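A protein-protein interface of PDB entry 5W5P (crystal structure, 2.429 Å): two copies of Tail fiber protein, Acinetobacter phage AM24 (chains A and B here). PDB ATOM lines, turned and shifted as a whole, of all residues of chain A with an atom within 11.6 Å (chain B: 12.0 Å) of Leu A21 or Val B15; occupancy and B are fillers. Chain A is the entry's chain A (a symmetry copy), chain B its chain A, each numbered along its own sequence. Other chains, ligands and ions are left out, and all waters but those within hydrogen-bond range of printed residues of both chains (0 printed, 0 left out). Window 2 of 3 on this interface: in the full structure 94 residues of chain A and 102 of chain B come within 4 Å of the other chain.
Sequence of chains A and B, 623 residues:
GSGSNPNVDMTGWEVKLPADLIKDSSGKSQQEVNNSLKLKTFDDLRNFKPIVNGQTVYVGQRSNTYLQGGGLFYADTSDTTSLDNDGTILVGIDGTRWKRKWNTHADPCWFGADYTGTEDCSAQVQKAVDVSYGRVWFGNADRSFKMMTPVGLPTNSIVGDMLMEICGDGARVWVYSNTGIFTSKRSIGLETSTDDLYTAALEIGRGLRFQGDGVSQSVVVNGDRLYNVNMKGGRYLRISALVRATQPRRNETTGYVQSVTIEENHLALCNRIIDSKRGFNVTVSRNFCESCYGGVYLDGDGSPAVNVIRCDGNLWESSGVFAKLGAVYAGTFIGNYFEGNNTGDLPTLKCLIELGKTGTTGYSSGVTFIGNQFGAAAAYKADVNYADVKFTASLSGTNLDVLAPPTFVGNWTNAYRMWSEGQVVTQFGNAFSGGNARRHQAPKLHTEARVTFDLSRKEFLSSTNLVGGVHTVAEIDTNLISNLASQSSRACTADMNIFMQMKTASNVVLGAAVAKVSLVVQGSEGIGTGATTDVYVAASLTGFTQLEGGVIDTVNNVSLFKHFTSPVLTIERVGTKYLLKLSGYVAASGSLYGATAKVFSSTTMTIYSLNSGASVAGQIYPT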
ATOM      1  N   VAL A  15       0.292 -37.951  32.818  1.00  0.00           N
ATOM      2  CA  VAL A  15       1.363 -36.949  32.795  1.00  0.00           C
ATOM      3  C   VAL A  15       0.917 -35.877  31.804  1.00  0.00           C
ATOM      4  O   VAL A  15       1.188 -35.953  30.606  1.00  0.00           O
ATOM      5  CB  VAL A  15       2.710 -37.564  32.421  1.00  0.00           C
ATOM      6  CG1 VAL A  15       3.796 -36.495  32.376  1.00  0.00           C
ATOM      7  CG2 VAL A  15       3.078 -38.679  33.396  1.00  0.00           C
ATOM      8  N   LYS A  16       0.216 -34.863  32.310  1.00  0.00           N
ATOM      9  CA  LYS A  16      -0.411 -33.854  31.465  1.00  0.00           C
ATOM     10  C   LYS A  16       0.022 -32.466  31.913  1.00  0.00           C
ATOM     11  O   LYS A  16      -0.260 -32.062  33.044  1.00  0.00           O
ATOM     12  CB  LYS A  16      -1.938 -33.973  31.506  1.00  0.00           C
ATOM     13  CG  LYS A  16      -2.470 -35.333  31.080  1.00  0.00           C
ATOM     14  CD  LYS A  16      -3.892 -35.554  31.574  1.00  0.00           C
ATOM     15  CE  LYS A  16      -4.659 -36.488  30.651  1.00  0.00           C
ATOM     16  NZ  LYS A  16      -5.713 -37.247  31.377  1.00  0.00           N
ATOM     17  N   LEU A  17       0.706 -31.745  31.026  1.00  0.00           N
ATOM     18  CA  LEU A  17       1.007 -30.334  31.225  1.00  0.00           C
ATOM     19  C   LEU A  17       0.147 -29.519  30.275  1.00  0.00           C
ATOM     20  O   LEU A  17       0.259 -29.700  29.053  1.00  0.00           O
ATOM     21  CB  LEU A  17       2.486 -30.042  30.977  1.00  0.00           C
ATOM     22  CG  LEU A  17       3.497 -30.307  32.091  1.00  0.00           C
ATOM     23  CD1 LEU A  17       4.719 -29.427  31.898  1.00  0.00           C
ATOM     24  CD2 LEU A  17       2.879 -30.081  33.459  1.00  0.00           C
ATOM     25  N   PRO A  18      -0.717 -28.633  30.764  1.00  0.00           N
ATOM     26  CA  PRO A  18      -1.549 -27.840  29.849  1.00  0.00           C
ATOM     27  C   PRO A  18      -0.698 -26.918  28.988  1.00  0.00           C
ATOM     28  O   PRO A  18       0.316 -26.380  29.434  1.00  0.00           O
ATOM     29  CB  PRO A  18      -2.465 -27.051  30.790  1.00  0.00           C
ATOM     30  CG  PRO A  18      -1.747 -27.041  32.103  1.00  0.00           C
ATOM     31  CD  PRO A  18      -1.001 -28.336  32.177  1.00  0.00           C
ATOM     32  N   ALA A  19      -1.122 -26.745  27.734  1.00  0.00           N
ATOM     33  CA  ALA A  19      -0.376 -25.903  26.806  1.00  0.00           C
ATOM     34  C   ALA A  19      -0.329 -24.448  27.251  1.00  0.00           C
ATOM     35  O   ALA A  19       0.595 -23.725  26.864  1.00  0.00           O
ATOM     36  CB  ALA A  19      -0.977 -26.001  25.404  1.00  0.00           C
ATOM     37  N   ASP A  20      -1.290 -24.006  28.065  1.00  0.00           N
ATOM     38  CA  ASP A  20      -1.267 -22.642  28.584  1.00  0.00           C
ATOM     39  C   ASP A  20      -0.081 -22.373  29.501  1.00  0.00           C
ATOM     40  O   ASP A  20       0.184 -21.209  29.817  1.00  0.00           O
ATOM     41  CB  ASP A  20      -2.569 -22.340  29.325  1.00  0.00           C
ATOM     42  CG  ASP A  20      -3.068 -20.930  29.068  1.00  0.00           C
ATOM     43  OD1 ASP A  20      -2.362 -19.968  29.448  1.00  0.00           O
ATOM     44  OD2 ASP A  20      -4.160 -20.784  28.475  1.00  0.00           O
ATOM     45  N   LEU A  21       0.634 -23.407  29.931  1.00  0.00           N
ATOM     46  CA  LEU A  21       1.804 -23.238  30.782  1.00  0.00           C
ATOM     47  C   LEU A  21       3.100 -23.167  29.988  1.00  0.00           C
ATOM     48  O   LEU A  21       4.173 -23.056  30.588  1.00  0.00           O
ATOM     49  CB  LEU A  21       1.885 -24.375  31.806  1.00  0.00           C
ATOM     50  CG  LEU A  21       1.130 -24.202  33.127  1.00  0.00           C
ATOM     51  CD1 LEU A  21      -0.301 -23.700  32.917  1.00  0.00           C
ATOM     52  CD2 LEU A  21       1.130 -25.510  33.896  1.00  0.00           C
ATOM     53  N   ILE A  22       3.026 -23.237  28.661  1.00  0.00           N
ATOM     54  CA  ILE A  22       4.181 -23.098  27.783  1.00  0.00           C
ATOM     55  C   ILE A  22       4.123 -21.719  27.140  1.00  0.00           C
ATOM     56  O   ILE A  22       3.061 -21.288  26.675  1.00  0.00           O
ATOM     57  CB  ILE A  22       4.214 -24.208  26.716  1.00  0.00           C
ATOM     58  CG1 ILE A  22       3.996 -25.580  27.362  1.00  0.00           C
ATOM     59  CG2 ILE A  22       5.511 -24.157  25.925  1.00  0.00           C
ATOM     60  CD1 ILE A  22       5.101 -25.993  28.314  1.00  0.00           C
ATOM     61  N   LYS A  23       5.262 -21.028  27.113  1.00  0.00           N
ATOM     62  CA  LYS A  23       5.350 -19.665  26.606  1.00  0.00           C
ATOM     63  C   LYS A  23       6.145 -19.642  25.307  1.00  0.00           C
ATOM     64  O   LYS A  23       7.262 -20.165  25.247  1.00  0.00           O
ATOM     65  CB  LYS A  23       6.002 -18.737  27.634  1.00  0.00           C
ATOM     66  CG  LYS A  23       6.115 -17.284  27.181  1.00  0.00           C
ATOM     67  CD  LYS A  23       7.053 -16.487  28.082  1.00  0.00           C
ATOM     68  CE  LYS A  23       6.608 -15.035  28.224  1.00  0.00           C
ATOM     69  NZ  LYS A  23       7.530 -14.271  29.116  1.00  0.00           N
ATOM     70  N   ASP A  24       5.565 -19.031  24.280  1.00  0.00           N
ATOM     71  CA  ASP A  24       6.213 -18.849  22.990  1.00  0.00           C
ATOM     72  C   ASP A  24       7.030 -17.564  23.016  1.00  0.00           C
ATOM     73  O   ASP A  24       6.729 -16.634  23.770  1.00  0.00           O
ATOM     74  CB  ASP A  24       5.158 -18.811  21.878  1.00  0.00           C
ATOM     75  CG  ASP A  24       5.722 -18.390  20.532  1.00  0.00           C
ATOM     76  OD1 ASP A  24       6.240 -19.265  19.805  1.00  0.00           O
ATOM     77  OD2 ASP A  24       5.625 -17.194  20.187  1.00  0.00           O
ATOM     78  N   SER A  25       8.080 -17.520  22.187  1.00  0.00           N
ATOM     79  CA  SER A  25       8.994 -16.378  22.198  1.00  0.00           C
ATOM     80  C   SER A  25       8.283 -15.048  21.965  1.00  0.00           C
ATOM     81  O   SER A  25       8.804 -14.005  22.371  1.00  0.00           O
ATOM     82  CB  SER A  25      10.097 -16.577  21.152  1.00  0.00           C
ATOM     83  OG  SER A  25       9.564 -16.782  19.859  1.00  0.00           O
ATOM     84  N   GLY A  27       5.776 -14.046  23.516  1.00  0.00           N
ATOM     85  CA  GLY A  27       5.158 -13.654  24.758  1.00  0.00           C
ATOM     86  C   GLY A  27       3.803 -14.281  25.008  1.00  0.00           C
ATOM     87  O   GLY A  27       3.323 -14.248  26.146  1.00  0.00           O
ATOM     88  N   LYS A  28       3.177 -14.846  23.981  1.00  0.00           N
ATOM     89  CA  LYS A  28       1.890 -15.506  24.133  1.00  0.00           C
ATOM     90  C   LYS A  28       2.087 -16.980  24.468  1.00  0.00           C
ATOM     91  O   LYS A  28       3.125 -17.579  24.176  1.00  0.00           O
ATOM     92  CB  LYS A  28       1.053 -15.354  22.860  1.00  0.00           C
ATOM     93  CG  LYS A  28       0.654 -13.916  22.562  1.00  0.00           C
ATOM     94  CD  LYS A  28      -0.774 -13.818  22.052  1.00  0.00           C
ATOM     95  CE  LYS A  28      -1.534 -12.698  22.749  1.00  0.00           C
ATOM     96  NZ  LYS A  28      -0.730 -11.446  22.833  1.00  0.00           N
ATOM     97  N   SER A  29       1.069 -17.563  25.093  1.00  0.00           N
ATOM     98  CA  SER A  29       1.160 -18.946  25.531  1.00  0.00           C
ATOM     99  C   SER A  29       1.076 -19.893  24.339  1.00  0.00           C
ATOM    100  O   SER A  29       0.621 -19.529  23.250  1.00  0.00           O
ATOM    101  CB  SER A  29       0.048 -19.269  26.529  1.00  0.00           C
ATOM    102  OG  SER A  29      -1.200 -19.416  25.875  1.00  0.00           O
ATOM    103  N   GLN A  30       1.526 -21.133  24.561  1.00  0.00           N
ATOM    104  CA  GLN A  30       1.405 -22.150  23.524  1.00  0.00           C
ATOM    105  C   GLN A  30      -0.051 -22.412  23.175  1.00  0.00           C
ATOM    106  O   GLN A  30      -0.371 -22.679  22.010  1.00  0.00           O
ATOM    107  CB  GLN A  30       2.078 -23.448  23.964  1.00  0.00           C
ATOM    108  CG  GLN A  30       2.008 -24.560  22.930  1.00  0.00           C
ATOM    109  CD  GLN A  30       2.847 -24.264  21.706  1.00  0.00           C
ATOM    110  OE1 GLN A  30       4.004 -23.865  21.820  1.00  0.00           O
ATOM    111  NE2 GLN A  30       2.265 -24.454  20.522  1.00  0.00           N
ATOM    112  N   GLN A  31      -0.946 -22.334  24.162  1.00  0.00           N
ATOM    113  CA  GLN A  31      -2.366 -22.497  23.875  1.00  0.00           C
ATOM    114  C   GLN A  31      -2.851 -21.451  22.878  1.00  0.00           C
ATOM    115  O   GLN A  31      -3.615 -21.770  21.963  1.00  0.00           O
ATOM    116  CB  GLN A  31      -3.181 -22.425  25.164  1.00  0.00           C
ATOM    117  CG  GLN A  31      -4.652 -22.743  24.966  1.00  0.00           C
ATOM    118  CD  GLN A  31      -4.867 -24.047  24.230  1.00  0.00           C
ATOM    119  OE1 GLN A  31      -4.543 -25.123  24.739  1.00  0.00           O
ATOM    120  NE2 GLN A  31      -5.412 -23.961  23.024  1.00  0.00           N
ATOM    121  N   GLU A  32      -2.407 -20.199  23.031  1.00  0.00           N
ATOM    122  CA  GLU A  32      -2.793 -19.158  22.080  1.00  0.00           C
ATOM    123  C   GLU A  32      -2.182 -19.399  20.703  1.00  0.00           C
ATOM    124  O   GLU A  32      -2.819 -19.109  19.684  1.00  0.00           O
ATOM    125  CB  GLU A  32      -2.387 -17.783  22.609  1.00  0.00           C
ATOM    126  CG  GLU A  32      -3.269 -17.264  23.727  1.00  0.00           C
ATOM    127  CD  GLU A  32      -2.569 -16.223  24.581  1.00  0.00           C
ATOM    128  OE1 GLU A  32      -1.457 -16.506  25.077  1.00  0.00           O
ATOM    129  OE2 GLU A  32      -3.128 -15.119  24.755  1.00  0.00           O
ATOM    130  N   VAL A  33      -0.954 -19.921  20.656  1.00  0.00           N
ATOM    131  CA  VAL A  33      -0.356 -20.316  19.384  1.00  0.00           C
ATOM    132  C   VAL A  33      -1.164 -21.438  18.747  1.00  0.00           C
ATOM    133  O   VAL A  33      -1.450 -21.414  17.544  1.00  0.00           O
ATOM    134  CB  VAL A  33       1.116 -20.726  19.593  1.00  0.00           C
ATOM    135  CG1 VAL A  33       1.568 -21.690  18.507  1.00  0.00           C
ATOM    136  CG2 VAL A  33       2.013 -19.500  19.637  1.00  0.00           C
ATOM    137  N   ASN A  34      -1.545 -22.445  19.541  1.00  0.00           N
ATOM    138  CA  ASN A  34      -2.348 -23.541  19.007  1.00  0.00           C
ATOM    139  C   ASN A  34      -3.693 -23.049  18.489  1.00  0.00           C
ATOM    140  O   ASN A  34      -4.208 -23.582  17.500  1.00  0.00           O
ATOM    141  CB  ASN A  34      -2.560 -24.617  20.074  1.00  0.00           C
ATOM    142  CG  ASN A  34      -1.279 -25.338  20.445  1.00  0.00           C
ATOM    143  OD1 ASN A  34      -0.219 -25.082  19.868  1.00  0.00           O
ATOM    144  ND2 ASN A  34      -1.367 -26.242  21.420  1.00  0.00           N
ATOM    145  N   ASN A  35      -4.267 -22.031  19.132  1.00  0.00           N
ATOM    146  CA  ASN A  35      -5.601 -21.572  18.761  1.00  0.00           C
ATOM    147  C   ASN A  35      -5.663 -21.009  17.348  1.00  0.00           C
ATOM    148  O   ASN A  35      -6.748 -20.983  16.758  1.00  0.00           O
ATOM    149  CB  ASN A  35      -6.091 -20.523  19.760  1.00  0.00           C
ATOM    150  CG  ASN A  35      -6.533 -21.140  21.072  1.00  0.00           C
ATOM    151  OD1 ASN A  35      -6.749 -22.351  21.160  1.00  0.00           O
ATOM    152  ND2 ASN A  35      -6.673 -20.309  22.102  1.00  0.00           N
ATOM    153  N   GLU B  14       3.765 -16.273  35.497  1.00  0.00           N
ATOM    154  CA  GLU B  14       4.596 -16.734  36.603  1.00  0.00           C
ATOM    155  C   GLU B  14       5.073 -18.168  36.381  1.00  0.00           C
ATOM    156  O   GLU B  14       6.263 -18.465  36.516  1.00  0.00           O
ATOM    157  CB  GLU B  14       3.833 -16.636  37.926  1.00  0.00           C
ATOM    158  CG  GLU B  14       4.731 -16.460  39.138  1.00  0.00           C
ATOM    159  CD  GLU B  14       3.950 -16.205  40.411  1.00  0.00           C
ATOM    160  OE1 GLU B  14       2.740 -15.901  40.317  1.00  0.00           O
ATOM    161  OE2 GLU B  14       4.547 -16.305  41.504  1.00  0.00           O
ATOM    162  N   VAL B  15       4.133 -19.051  36.048  1.00  0.00           N
ATOM    163  CA  VAL B  15       4.442 -20.445  35.715  1.00  0.00           C
ATOM    164  C   VAL B  15       4.675 -20.479  34.207  1.00  0.00           C
ATOM    165  O   VAL B  15       3.752 -20.668  33.416  1.00  0.00           O
ATOM    166  CB  VAL B  15       3.331 -21.397  36.154  1.00  0.00           C
ATOM    167  CG1 VAL B  15       3.668 -22.833  35.768  1.00  0.00           C
ATOM    168  CG2 VAL B  15       3.085 -21.275  37.655  1.00  0.00           C
ATOM    169  N   LYS B  16       5.929 -20.284  33.801  1.00  0.00           N
ATOM    170  CA  LYS B  16       6.275 -20.128  32.393  1.00  0.00           C
ATOM    171  C   LYS B  16       7.367 -21.118  32.018  1.00  0.00           C
ATOM    172  O   LYS B  16       8.474 -21.056  32.560  1.00  0.00           O
ATOM    173  CB  LYS B  16       6.729 -18.696  32.092  1.00  0.00           C
ATOM    174  CG  LYS B  16       5.702 -17.629  32.441  1.00  0.00           C
ATOM    175  CD  LYS B  16       6.348 -16.257  32.571  1.00  0.00           C
ATOM    176  CE  LYS B  16       5.365 -15.149  32.227  1.00  0.00           C
ATOM    177  NZ  LYS B  16       5.674 -13.886  32.953  1.00  0.00           N
ATOM    178  N   LEU B  17       7.052 -22.026  31.096  1.00  0.00           N
ATOM    179  CA  LEU B  17       8.042 -22.901  30.484  1.00  0.00           C
ATOM    180  C   LEU B  17       8.264 -22.450  29.052  1.00  0.00           C
ATOM    181  O   LEU B  17       7.307 -22.450  28.263  1.00  0.00           O
ATOM    182  CB  LEU B  17       7.586 -24.358  30.513  1.00  0.00           C
ATOM    183  CG  LEU B  17       7.795 -25.183  31.781  1.00  0.00           C
ATOM    184  CD1 LEU B  17       7.862 -26.659  31.431  1.00  0.00           C
ATOM    185  CD2 LEU B  17       9.048 -24.747  32.520  1.00  0.00           C
ATOM    186  N   PRO B  18       9.474 -22.055  28.665  1.00  0.00           N
ATOM    187  CA  PRO B  18       9.695 -21.620  27.280  1.00  0.00           C
ATOM    188  C   PRO B  18       9.478 -22.765  26.301  1.00  0.00           C
ATOM    189  O   PRO B  18       9.798 -23.920  26.585  1.00  0.00           O
ATOM    190  CB  PRO B  18      11.151 -21.145  27.281  1.00  0.00           C
ATOM    191  CG  PRO B  18      11.776 -21.824  28.459  1.00  0.00           C
ATOM    192  CD  PRO B  18      10.693 -21.951  29.485  1.00  0.00           C
ATOM    193  N   ALA B  19       8.920 -22.430  25.136  1.00  0.00           N
ATOM    194  CA  ALA B  19       8.640 -23.445  24.126  1.00  0.00           C
ATOM    195  C   ALA B  19       9.905 -24.114  23.608  1.00  0.00           C
ATOM    196  O   ALA B  19       9.837 -25.250  23.126  1.00  0.00           O
ATOM    197  CB  ALA B  19       7.859 -22.832  22.964  1.00  0.00           C
ATOM    198  N   ASP B  20      11.057 -23.448  23.708  1.00  0.00           N
ATOM    199  CA  ASP B  20      12.316 -24.058  23.294  1.00  0.00           C
ATOM    200  C   ASP B  20      12.702 -25.263  24.141  1.00  0.00           C
ATOM    201  O   ASP B  20      13.613 -26.004  23.755  1.00  0.00           O
ATOM    202  CB  ASP B  20      13.439 -23.022  23.332  1.00  0.00           C
ATOM    203  CG  ASP B  20      14.399 -23.164  22.164  1.00  0.00           C
ATOM    204  OD1 ASP B  20      15.065 -24.218  22.065  1.00  0.00           O
ATOM    205  OD2 ASP B  20      14.475 -22.226  21.339  1.00  0.00           O
ATOM    206  N   LEU B  21      12.041 -25.480  25.272  1.00  0.00           N
ATOM    207  CA  LEU B  21      12.321 -26.627  26.124  1.00  0.00           C
ATOM    208  C   LEU B  21      11.418 -27.815  25.822  1.00  0.00           C
ATOM    209  O   LEU B  21      11.528 -28.845  26.493  1.00  0.00           O
ATOM    210  CB  LEU B  21      12.186 -26.238  27.601  1.00  0.00           C
ATOM    211  CG  LEU B  21      13.417 -25.652  28.300  1.00  0.00           C
ATOM    212  CD1 LEU B  21      14.099 -24.566  27.463  1.00  0.00           C
ATOM    213  CD2 LEU B  21      13.028 -25.112  29.663  1.00  0.00           C
ATOM    214  N   ILE B  22      10.530 -27.692  24.839  1.00  0.00           N
ATOM    215  CA  ILE B  22       9.667 -28.780  24.395  1.00  0.00           C
ATOM    216  C   ILE B  22      10.206 -29.301  23.069  1.00  0.00           C
ATOM    217  O   ILE B  22      10.550 -28.513  22.180  1.00  0.00           O
ATOM    218  CB  ILE B  22       8.205 -28.318  24.257  1.00  0.00           C
ATOM    219  CG1 ILE B  22       7.764 -27.550  25.508  1.00  0.00           C
ATOM    220  CG2 ILE B  22       7.291 -29.498  23.969  1.00  0.00           C
ATOM    221  CD1 ILE B  22       7.735 -28.393  26.768  1.00  0.00           C
ATOM    222  N   GLN B  30       9.790 -27.149  20.080  1.00  0.00           N
ATOM    223  CA  GLN B  30       8.461 -26.587  19.869  1.00  0.00           C
ATOM    224  C   GLN B  30       8.541 -25.151  19.377  1.00  0.00           C
ATOM    225  O   GLN B  30       7.706 -24.726  18.569  1.00  0.00           O
ATOM    226  CB  GLN B  30       7.639 -26.654  21.155  1.00  0.00           C
ATOM    227  CG  GLN B  30       6.231 -26.098  21.016  1.00  0.00           C
ATOM    228  CD  GLN B  30       5.356 -26.959  20.133  1.00  0.00           C
ATOM    229  OE1 GLN B  30       5.317 -28.179  20.286  1.00  0.00           O
ATOM    230  NE2 GLN B  30       4.648 -26.330  19.196  1.00  0.00           N
ATOM    231  N   GLN B  31       9.536 -24.393  19.842  1.00  0.00           N
ATOM    232  CA  GLN B  31       9.711 -23.033  19.348  1.00  0.00           C
ATOM    233  C   GLN B  31       9.935 -23.019  17.841  1.00  0.00           C
ATOM    234  O   GLN B  31       9.376 -22.174  17.135  1.00  0.00           O
ATOM    235  CB  GLN B  31      10.872 -22.351  20.068  1.00  0.00           C
ATOM    236  CG  GLN B  31      11.017 -20.881  19.719  1.00  0.00           C
ATOM    237  CD  GLN B  31       9.721 -20.118  19.883  1.00  0.00           C
ATOM    238  OE1 GLN B  31       9.211 -19.965  20.996  1.00  0.00           O
ATOM    239  NE2 GLN B  31       9.174 -19.637  18.773  1.00  0.00           N
ATOM    240  N   ASN B  34       6.647 -23.715  16.248  1.00  0.00           N
ATOM    241  CA  ASN B  34       5.820 -22.512  16.286  1.00  0.00           C
ATOM    242  C   ASN B  34       6.265 -21.494  15.245  1.00  0.00           C
ATOM    243  O   ASN B  34       5.429 -20.782  14.678  1.00  0.00           O
ATOM    244  CB  ASN B  34       5.854 -21.884  17.681  1.00  0.00           C
ATOM    245  CG  ASN B  34       5.177 -22.745  18.730  1.00  0.00           C
ATOM    246  OD1 ASN B  34       4.622 -23.802  18.420  1.00  0.00           O
ATOM    247  ND2 ASN B  34       5.227 -22.300  19.986  1.00  0.00           N
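Of the 12 printed residues of chain B, 9 touch a printed residue of chain A. Printed residues of chain B that touch a printed residue of chain A: Val B15, Lys B16, Leu B17, Pro B18, Ala B19, Ile B22, Gln B30, Gln B31 and Asn B34. Hydrophobic or aromatic side chains of chain B within 4 Å of the printed part of chain A: Val B15, Leu B17, Ala B19 and Ile B22. Printed residues of chain A that touch a printed residue of chain B: Leu A21, Ile A22, Lys A23, Asp A24, Ser A25, Gln A30 and Val A33. Among the printed residues, no Asp or Glu carboxylate lies within 4 Å of a Lys or Arg side-chain nitrogen of the other chain.
Among the printed residues, merely in contact across the chains: Leu A21 with Val B15, Ile A22 with Leu B17, Ile A22 with Ala B19, Ile A22 with Ile B22, Lys A23 with Lys B16, Lys A23 with Pro B18 and Val A33 with Asn B34.
Leu A21 touches Val B15, but with the chains exchanged Val A15 does not touch Leu B21 (12.4 Å). Leu A21 touches Leu B17, but with the chains exchanged Leu A17 does not touch Leu B21 (8.7 Å). Ile A22 touches Ala B19, but with the chains exchanged Ala A19 does not touch Ile B22 (8.2 Å). Ile B22 touches its own counterpart, Ile A22. 11 positions are printed for both chains.
Of the printed residues of chain B, Leu A21 touches Val B15 (3.7 Å) and Leu B17 (3.1 Å). Val B15 touches just one residue of chain A: Leu A21 (3.7 Å). No residue of chain B comes within 4 Å of Leu A17. No residue of chain B comes within 4 Å of Pro A18. Ala A19 touches none of the printed residues of chain B. No residue of chain B comes within 4 Å of Asp A20. Ile A22 touches just these residues of chain B: Leu B17, Ala B19 and Ile B22. No residue of chain B comes within 4 Å of Ser A29. No residue of chain A comes within 4 Å of Glu B14. Printed residues of chain B within 4 Å of Gln A30: Gln B30 and Asn B34. Printed residues of chain A within 4 Å of Lys B16: Lys A23 (3.9 Å). Of the printed residues of chain A, Gln B31 touches Asp A24 (3.1 Å) and Ser A25 (2.9 Å). Of the printed residues of chain A, Ile B22 touches Ile A22. Val A15 touches none of the printed residues of chain B. The nearest residue of chain A that does not touch Val B15 is Asp A20 (5.1 Å). The nearest printed residue of chain B that does not touch Gln A30 is Ala B19 (4.2 Å).
The backbone NH (N) of Leu B17 lies within hydrogen-bond range of the backbone carbonyl oxygen (O) of Leu A21. N of Lys A23 lies within hydrogen-bond range of O of Leu B17, at 2.7 Å. The backbone carbonyl oxygen (O) of Lys A23 lies within hydrogen-bond range of the backbone NH (N) of Ala B19 (2.8 Å). NE2 of Gln B30 sits close to NE2 of Gln A30. The side-chain amide nitrogen (NE2) of Gln B31 sits at hydrogen-bond distance from the side-chain carboxylate (OD1) of Asp A24, 3.1 Å away. The backbone NH (N) of Ser A25 is in hydrogen-bond range of the side-chain amide oxygen (OE1) of Gln B31 (2.9 Å). The side-chain amide nitrogen of Asn B34 lies within hydrogen-bond range of the side-chain carboxylate of Asp A24. ND2 of Asn B34 lies within hydrogen-bond range of OE1 of Gln A30.
The backbone NH (N) of Gln B31 is in hydrogen-bond range of the backbone carbonyl oxygen (O) of Ala B19 (3.4 Å). The backbone carbonyl oxygen (O) of Ile B22 lies within hydrogen-bond range of the backbone NH (N) of Gln B30. The side-chain amide nitrogen (NE2) of Gln B30 sits at hydrogen-bond distance from the side-chain amide oxygen (OD1) of Asn B34 (2.6 Å). The backbone NH (N) of Gln A30 sits at hydrogen-bond distance from the backbone carbonyl oxygen (O) of Ile A22 (2.6 Å). NE2 of Gln A30 is in hydrogen-bond range of OD1 of Asn A34 (2.6 Å).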
